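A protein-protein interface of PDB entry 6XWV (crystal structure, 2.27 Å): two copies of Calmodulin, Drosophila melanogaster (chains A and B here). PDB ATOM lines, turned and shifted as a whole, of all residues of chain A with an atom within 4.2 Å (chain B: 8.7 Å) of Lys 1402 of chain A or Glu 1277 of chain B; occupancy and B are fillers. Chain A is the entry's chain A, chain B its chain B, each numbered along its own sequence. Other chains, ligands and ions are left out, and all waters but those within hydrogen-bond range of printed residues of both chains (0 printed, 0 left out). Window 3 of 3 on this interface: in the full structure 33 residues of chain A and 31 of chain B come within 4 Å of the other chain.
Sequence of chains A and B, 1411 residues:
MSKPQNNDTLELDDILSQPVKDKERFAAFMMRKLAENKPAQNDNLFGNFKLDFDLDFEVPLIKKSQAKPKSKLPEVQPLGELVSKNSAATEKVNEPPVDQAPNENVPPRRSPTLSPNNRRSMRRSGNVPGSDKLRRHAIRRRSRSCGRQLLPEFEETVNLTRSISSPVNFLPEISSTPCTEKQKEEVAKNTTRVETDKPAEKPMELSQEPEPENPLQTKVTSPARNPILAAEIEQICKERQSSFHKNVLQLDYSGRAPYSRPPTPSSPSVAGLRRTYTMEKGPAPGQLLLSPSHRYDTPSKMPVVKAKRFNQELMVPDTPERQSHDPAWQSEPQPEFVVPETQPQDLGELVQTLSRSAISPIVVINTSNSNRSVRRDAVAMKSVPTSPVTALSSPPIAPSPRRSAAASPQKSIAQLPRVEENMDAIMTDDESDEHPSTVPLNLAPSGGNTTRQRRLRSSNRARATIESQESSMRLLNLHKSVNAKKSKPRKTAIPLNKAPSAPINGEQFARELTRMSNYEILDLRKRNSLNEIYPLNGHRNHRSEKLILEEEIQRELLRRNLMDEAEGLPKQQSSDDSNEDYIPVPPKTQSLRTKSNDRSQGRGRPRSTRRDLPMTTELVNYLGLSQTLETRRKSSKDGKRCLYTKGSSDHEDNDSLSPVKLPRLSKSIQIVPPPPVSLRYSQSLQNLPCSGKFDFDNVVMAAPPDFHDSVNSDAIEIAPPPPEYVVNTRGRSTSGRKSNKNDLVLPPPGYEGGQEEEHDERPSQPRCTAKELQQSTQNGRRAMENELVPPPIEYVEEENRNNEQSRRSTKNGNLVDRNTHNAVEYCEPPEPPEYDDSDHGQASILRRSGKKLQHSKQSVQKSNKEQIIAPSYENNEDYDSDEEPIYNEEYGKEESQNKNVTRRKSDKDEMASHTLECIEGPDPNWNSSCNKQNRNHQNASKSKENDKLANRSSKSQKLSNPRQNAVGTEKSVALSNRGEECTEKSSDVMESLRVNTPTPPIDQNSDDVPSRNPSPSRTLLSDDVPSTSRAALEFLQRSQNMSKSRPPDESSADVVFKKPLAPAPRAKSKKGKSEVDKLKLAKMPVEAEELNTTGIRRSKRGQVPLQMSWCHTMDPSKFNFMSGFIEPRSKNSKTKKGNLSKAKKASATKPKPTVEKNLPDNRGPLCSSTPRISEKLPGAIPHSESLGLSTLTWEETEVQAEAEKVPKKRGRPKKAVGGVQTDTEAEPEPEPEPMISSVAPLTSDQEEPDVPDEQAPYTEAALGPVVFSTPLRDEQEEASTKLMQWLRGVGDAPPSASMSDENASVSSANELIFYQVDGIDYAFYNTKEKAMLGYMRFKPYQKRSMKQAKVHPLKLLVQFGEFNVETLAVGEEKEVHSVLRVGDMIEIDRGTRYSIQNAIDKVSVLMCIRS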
ATOM      1  N   ARG A1288     -13.547  -2.856  23.931  1.00  0.00           N
ATOM      2  CA  ARG A1288     -14.657  -2.242  23.214  1.00  0.00           C
ATOM      3  C   ARG A1288     -14.715  -2.668  21.752  1.00  0.00           C
ATOM      4  O   ARG A1288     -15.665  -2.307  21.051  1.00  0.00           O
ATOM      5  CB  ARG A1288     -14.566  -0.721  23.321  1.00  0.00           C
ATOM      6  CG  ARG A1288     -15.343  -0.159  24.484  1.00  0.00           C
ATOM      7  CD  ARG A1288     -14.873   1.236  24.798  1.00  0.00           C
ATOM      8  NE  ARG A1288     -15.617   2.224  24.025  1.00  0.00           N
ATOM      9  CZ  ARG A1288     -15.137   3.410  23.673  1.00  0.00           C
ATOM     10  NH1 ARG A1288     -13.907   3.762  24.027  1.00  0.00           N
ATOM     11  NH2 ARG A1288     -15.891   4.246  22.972  1.00  0.00           N
ATOM     12  N   PRO A1340     -24.711  -2.295  20.400  1.00  0.00           N
ATOM     13  CA  PRO A1340     -25.745  -1.325  20.801  1.00  0.00           C
ATOM     14  C   PRO A1340     -27.124  -1.933  21.071  1.00  0.00           C
ATOM     15  O   PRO A1340     -27.723  -2.577  20.194  1.00  0.00           O
ATOM     16  CB  PRO A1340     -25.805  -0.376  19.609  1.00  0.00           C
ATOM     17  CG  PRO A1340     -24.435  -0.368  19.085  1.00  0.00           C
ATOM     18  CD  PRO A1340     -23.899  -1.779  19.283  1.00  0.00           C
ATOM     19  N   PHE A1360     -17.330  -0.899  30.893  1.00  0.00           N
ATOM     20  CA  PHE A1360     -17.568   0.290  30.086  1.00  0.00           C
ATOM     21  C   PHE A1360     -19.027   0.295  29.650  1.00  0.00           C
ATOM     22  O   PHE A1360     -19.594  -0.760  29.357  1.00  0.00           O
ATOM     23  CB  PHE A1360     -16.644   0.331  28.861  1.00  0.00           C
ATOM     24  CG  PHE A1360     -16.821   1.560  28.004  1.00  0.00           C
ATOM     25  CD1 PHE A1360     -16.083   2.709  28.251  1.00  0.00           C
ATOM     26  CD2 PHE A1360     -17.718   1.563  26.948  1.00  0.00           C
ATOM     27  CE1 PHE A1360     -16.243   3.838  27.461  1.00  0.00           C
ATOM     28  CE2 PHE A1360     -17.882   2.685  26.160  1.00  0.00           C
ATOM     29  CZ  PHE A1360     -17.143   3.823  26.415  1.00  0.00           C
ATOM     30  N   ASN A1398     -27.719  -4.199  26.896  1.00  0.00           N
ATOM     31  CA  ASN A1398     -26.973  -2.965  26.687  1.00  0.00           C
ATOM     32  C   ASN A1398     -27.952  -1.796  26.639  1.00  0.00           C
ATOM     33  O   ASN A1398     -28.901  -1.808  25.850  1.00  0.00           O
ATOM     34  CB  ASN A1398     -26.162  -3.055  25.397  1.00  0.00           C
ATOM     35  CG  ASN A1398     -25.192  -1.899  25.236  1.00  0.00           C
ATOM     36  OD1 ASN A1398     -25.177  -0.969  26.042  1.00  0.00           O
ATOM     37  ND2 ASN A1398     -24.372  -1.956  24.193  1.00  0.00           N
ATOM     38  N   ILE A1400     -27.464   1.438  25.883  1.00  0.00           N
ATOM     39  CA  ILE A1400     -27.134   2.589  25.050  1.00  0.00           C
ATOM     40  C   ILE A1400     -26.831   2.151  23.621  1.00  0.00           C
ATOM     41  O   ILE A1400     -26.771   0.963  23.301  1.00  0.00           O
ATOM     42  CB  ILE A1400     -25.951   3.394  25.619  1.00  0.00           C
ATOM     43  CG1 ILE A1400     -24.735   2.488  25.807  1.00  0.00           C
ATOM     44  CG2 ILE A1400     -26.348   4.051  26.933  1.00  0.00           C
ATOM     45  CD1 ILE A1400     -23.571   3.160  26.507  1.00  0.00           C
ATOM     46  N   ASP A1401     -26.627   3.156  22.758  1.00  0.00           N
ATOM     47  CA  ASP A1401     -26.351   2.982  21.335  1.00  0.00           C
ATOM     48  C   ASP A1401     -24.849   2.888  21.047  1.00  0.00           C
ATOM     49  O   ASP A1401     -24.382   3.289  19.967  1.00  0.00           O
ATOM     50  CB  ASP A1401     -27.017   4.122  20.551  1.00  0.00           C
ATOM     51  CG  ASP A1401     -26.955   3.939  19.038  1.00  0.00           C
ATOM     52  OD1 ASP A1401     -27.709   3.101  18.505  1.00  0.00           O
ATOM     53  OD2 ASP A1401     -26.161   4.650  18.388  1.00  0.00           O
ATOM     54  N   LYS A1402     -24.082   2.388  22.013  1.00  0.00           N
ATOM     55  CA  LYS A1402     -22.653   2.166  21.866  1.00  0.00           C
ATOM     56  C   LYS A1402     -22.332   0.775  22.376  1.00  0.00           C
ATOM     57  O   LYS A1402     -23.132   0.144  23.072  1.00  0.00           O
ATOM     58  CB  LYS A1402     -21.820   3.194  22.638  1.00  0.00           C
ATOM     59  CG  LYS A1402     -21.764   4.545  22.003  1.00  0.00           C
ATOM     60  CD  LYS A1402     -20.899   5.493  22.830  1.00  0.00           C
ATOM     61  CE  LYS A1402     -21.069   5.265  24.318  1.00  0.00           C
ATOM     62  NZ  LYS A1402     -21.380   6.548  25.008  1.00  0.00           N
ATOM     63  N   VAL A1403     -21.125   0.314  22.050  1.00  0.00           N
ATOM     64  CA  VAL A1403     -20.656  -0.948  22.595  1.00  0.00           C
ATOM     65  C   VAL A1403     -20.506  -0.787  24.098  1.00  0.00           C
ATOM     66  O   VAL A1403     -19.956   0.209  24.584  1.00  0.00           O
ATOM     67  CB  VAL A1403     -19.334  -1.366  21.932  1.00  0.00           C
ATOM     68  CG1 VAL A1403     -18.665  -2.459  22.735  1.00  0.00           C
ATOM     69  CG2 VAL A1403     -19.581  -1.816  20.505  1.00  0.00           C
ATOM     70  N   SER A1404     -21.019  -1.753  24.846  1.00  0.00           N
ATOM     71  CA  SER A1404     -20.869  -1.790  26.291  1.00  0.00           C
ATOM     72  C   SER A1404     -20.169  -3.087  26.660  1.00  0.00           C
ATOM     73  O   SER A1404     -20.379  -4.122  26.013  1.00  0.00           O
ATOM     74  CB  SER A1404     -22.220  -1.696  26.996  1.00  0.00           C
ATOM     75  OG  SER A1404     -22.608  -0.348  27.185  1.00  0.00           O
ATOM     76  N   ASP B1274     -19.158  10.138  23.824  1.00  0.00           N
ATOM     77  CA  ASP B1274     -18.300  10.938  24.683  1.00  0.00           C
ATOM     78  C   ASP B1274     -18.692  10.801  26.154  1.00  0.00           C
ATOM     79  O   ASP B1274     -17.832  10.635  27.014  1.00  0.00           O
ATOM     80  CB  ASP B1274     -18.332  12.411  24.256  1.00  0.00           C
ATOM     81  CG  ASP B1274     -17.120  12.798  23.423  1.00  0.00           C
ATOM     82  OD1 ASP B1274     -17.128  13.890  22.813  1.00  0.00           O
ATOM     83  OD2 ASP B1274     -16.147  12.010  23.394  1.00  0.00           O
ATOM     84  N   GLU B1275     -19.997  10.789  26.430  1.00  0.00           N
ATOM     85  CA  GLU B1275     -20.469  10.733  27.812  1.00  0.00           C
ATOM     86  C   GLU B1275     -19.953   9.500  28.557  1.00  0.00           C
ATOM     87  O   GLU B1275     -19.527   9.603  29.714  1.00  0.00           O
ATOM     88  CB  GLU B1275     -21.997  10.771  27.830  1.00  0.00           C
ATOM     89  CG  GLU B1275     -22.642  10.579  29.200  1.00  0.00           C
ATOM     90  CD  GLU B1275     -24.163  10.580  29.140  1.00  0.00           C
ATOM     91  OE1 GLU B1275     -24.794  10.584  30.217  1.00  0.00           O
ATOM     92  OE2 GLU B1275     -24.728  10.573  28.024  1.00  0.00           O
ATOM     93  N   GLN B1276     -20.013   8.317  27.926  1.00  0.00           N
ATOM     94  CA  GLN B1276     -19.541   7.093  28.586  1.00  0.00           C
ATOM     95  C   GLN B1276     -18.020   7.029  28.699  1.00  0.00           C
ATOM     96  O   GLN B1276     -17.495   6.663  29.759  1.00  0.00           O
ATOM     97  CB  GLN B1276     -20.046   5.855  27.848  1.00  0.00           C
ATOM     98  CG  GLN B1276     -21.258   5.190  28.453  1.00  0.00           C
ATOM     99  CD  GLN B1276     -22.449   6.117  28.561  1.00  0.00           C
ATOM    100  OE1 GLN B1276     -22.786   6.835  27.616  1.00  0.00           O
ATOM    101  NE2 GLN B1276     -23.125   6.073  29.702  1.00  0.00           N
ATOM    102  N   GLU B1277     -17.301   7.404  27.637  1.00  0.00           N
ATOM    103  CA  GLU B1277     -15.850   7.450  27.733  1.00  0.00           C
ATOM    104  C   GLU B1277     -15.418   8.466  28.769  1.00  0.00           C
ATOM    105  O   GLU B1277     -14.427   8.258  29.467  1.00  0.00           O
ATOM    106  CB  GLU B1277     -15.206   7.855  26.410  1.00  0.00           C
ATOM    107  CG  GLU B1277     -15.685   7.236  25.139  1.00  0.00           C
ATOM    108  CD  GLU B1277     -16.981   7.810  24.589  1.00  0.00           C
ATOM    109  OE1 GLU B1277     -18.023   7.784  25.278  1.00  0.00           O
ATOM    110  OE2 GLU B1277     -16.974   8.230  23.411  1.00  0.00           O
ATOM    111  N   GLU B1278     -16.100   9.606  28.824  1.00  0.00           N
ATOM    112  CA  GLU B1278     -15.780  10.645  29.777  1.00  0.00           C
ATOM    113  C   GLU B1278     -16.184  10.201  31.198  1.00  0.00           C
ATOM    114  O   GLU B1278     -15.614  10.691  32.182  1.00  0.00           O
ATOM    115  CB  GLU B1278     -16.315  11.943  29.092  1.00  0.00           C
ATOM    116  CG  GLU B1278     -15.942  13.363  29.587  1.00  0.00           C
ATOM    117  CD  GLU B1278     -16.917  14.348  28.884  1.00  0.00           C
ATOM    118  OE1 GLU B1278     -17.823  14.960  29.517  1.00  0.00           O
ATOM    119  OE2 GLU B1278     -16.734  14.516  27.665  1.00  0.00           O
ATOM    120  N   ALA B1279     -17.235   9.371  31.333  1.00  0.00           N
ATOM    121  CA  ALA B1279     -17.583   8.836  32.662  1.00  0.00           C
ATOM    122  C   ALA B1279     -16.572   7.796  33.162  1.00  0.00           C
ATOM    123  O   ALA B1279     -16.258   7.741  34.362  1.00  0.00           O
ATOM    124  CB  ALA B1279     -18.971   8.193  32.691  1.00  0.00           C
ATOM    125  N   SER B1280     -16.074   6.936  32.264  1.00  0.00           N
ATOM    126  CA  SER B1280     -15.105   5.914  32.663  1.00  0.00           C
ATOM    127  C   SER B1280     -13.791   6.544  33.107  1.00  0.00           C
ATOM    128  O   SER B1280     -13.139   6.053  34.036  1.00  0.00           O
ATOM    129  CB  SER B1280     -14.870   4.910  31.528  1.00  0.00           C
ATOM    130  OG  SER B1280     -14.298   5.530  30.394  1.00  0.00           O
ATOM    131  N   THR B1281     -13.390   7.630  32.450  1.00  0.00           N
ATOM    132  CA  THR B1281     -12.145   8.285  32.819  1.00  0.00           C
ATOM    133  C   THR B1281     -12.226   8.854  34.228  1.00  0.00           C
ATOM    134  O   THR B1281     -11.252   8.783  34.982  1.00  0.00           O
ATOM    135  CB  THR B1281     -11.821   9.383  31.805  1.00  0.00           C
ATOM    136  OG1 THR B1281     -11.419   8.786  30.565  1.00  0.00           O
ATOM    137  CG2 THR B1281     -10.702  10.284  32.316  1.00  0.00           C
ATOM    138  N   LYS B1282     -13.399   9.342  34.643  1.00  0.00           N
ATOM    139  CA  LYS B1282     -13.484   9.924  35.981  1.00  0.00           C
ATOM    140  C   LYS B1282     -13.468   8.864  37.071  1.00  0.00           C
ATOM    141  O   LYS B1282     -13.018   9.139  38.189  1.00  0.00           O
ATOM    142  CB  LYS B1282     -14.742  10.773  36.126  1.00  0.00           C
ATOM    143  CG  LYS B1282     -15.037  11.702  34.968  1.00  0.00           C
ATOM    144  CD  LYS B1282     -13.907  12.680  34.728  1.00  0.00           C
ATOM    145  CE  LYS B1282     -14.456  14.064  34.415  1.00  0.00           C
ATOM    146  NZ  LYS B1282     -13.760  15.126  35.201  1.00  0.00           N
ATOM    147  N   LEU B1283     -13.903   7.643  36.758  1.00  0.00           N
ATOM    148  CA  LEU B1283     -13.769   6.563  37.727  1.00  0.00           C
ATOM    149  C   LEU B1283     -12.306   6.196  37.934  1.00  0.00           C
ATOM    150  O   LEU B1283     -11.860   6.008  39.074  1.00  0.00           O
ATOM    151  CB  LEU B1283     -14.571   5.344  37.289  1.00  0.00           C
ATOM    152  CG  LEU B1283     -14.508   4.194  38.299  1.00  0.00           C
ATOM    153  CD1 LEU B1283     -15.089   4.638  39.634  1.00  0.00           C
ATOM    154  CD2 LEU B1283     -15.227   2.973  37.776  1.00  0.00           C
ATOM    155  N   MET B1284     -11.546   6.095  36.842  1.00  0.00           N
ATOM    156  CA  MET B1284     -10.121   5.799  36.948  1.00  0.00           C
ATOM    157  C   MET B1284      -9.411   6.865  37.774  1.00  0.00           C
ATOM    158  O   MET B1284      -8.607   6.549  38.660  1.00  0.00           O
ATOM    159  CB  MET B1284      -9.505   5.688  35.551  1.00  0.00           C
ATOM    160  CG  MET B1284      -8.163   4.969  35.498  1.00  0.00           C
ATOM    161  SD  MET B1284      -8.110   3.415  36.415  1.00  0.00           S
ATOM    162  CE  MET B1284      -9.151   2.372  35.394  1.00  0.00           C
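Arg 1288 of chain A touches Glu 1277 of chain B. CZ of Phe 1360 of chain A touches CB of Gln 1276 of chain B, 3.8 Å away. Phe 1360 of chain A touches Glu 1277 of chain B (CE1 to CA, 3.6 Å). OG of Ser 1280 of chain B touches CE1 of Phe 1360 of chain A, 3.9 Å away. CD1 of Ile 1400 of chain A touches CG of Gln 1276 of chain B, 3.6 Å away.
No position is printed for both chains. Of the 7 pairs that touch across the chains among the printed residues, none has its exchanged pair printed and touching as well.
OD1 of Asn 1398 of chain A sits at hydrogen-bond distance from N of Ile 1400 of chain A, 3.3 Å away. The side-chain amide nitrogen of Asn 1398 of chain A is in hydrogen-bond range of the backbone carbonyl oxygen of Lys 1402 of chain A (2.7 Å). The backbone NH (N) of Asp 1274 of chain B lies within hydrogen-bond range of the side-chain carboxylate (OE2) of Glu 1277 of chain B, 2.9 Å away. The backbone carbonyl oxygen (O) of Gln 1276 of chain B lies within hydrogen-bond range of the side-chain hydroxyl (OG) of Ser 1280 of chain B (3.5 Å). The backbone carbonyl oxygen (O) of Glu 1277 of chain B is in hydrogen-bond range of the side-chain hydroxyl (OG) of Ser 1280 of chain B (2.9 Å). The backbone carbonyl oxygen of Glu 1277 of chain B is in hydrogen-bond range of the side-chain hydroxyl of Thr 1281 of chain B, at 3.2 Å.
NZ of Lys 1402 of chain A lies within hydrogen-bond range of OE1 of Gln 1276 of chain B (3.0 Å). OE1 of Glu 1277 of chain B is in salt-bridge range of NZ of Lys 1402 of chain A (3.6 Å).
Of the 11 printed residues of chain B, 3 touch a printed residue of chain A. Of the 9 printed residues of chain A, 4 touch a printed residue of chain B. Among the printed residues, 7 pairs touch across the chains.
Of the printed residues of chain B, Arg 1288 of chain A touches Glu 1277 (3.7 Å). Of the printed residues of chain B, Phe 1360 of chain A touches Gln 1276 (3.8 Å), Glu 1277 (3.6 Å) and Ser 1280 (3.9 Å). Of the printed residues of chain B, Ile 1400 of chain A touches Gln 1276. Of chain B, only Gln 1276 and Glu 1277 come within 4 Å of Lys 1402 of chain A. Of the printed residues of chain A, Glu 1277 of chain B touches Arg 1288 (3.7 Å), Phe 1360 (3.6 Å) and Lys 1402 (3.6 Å). Printed residues of chain A within 4 Å of Ser 1280 of chain B: Phe 1360. Lys 1282 of chain B touches none of the printed residues of chain A. The nearest residue of chain B that does not touch Lys 1402 of chain A is Asp 1274 of chain B (4.4 Å). The nearest printed residue of chain A that does not touch Glu 1277 of chain B is Ile 1400 of chain A (7.3 Å).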
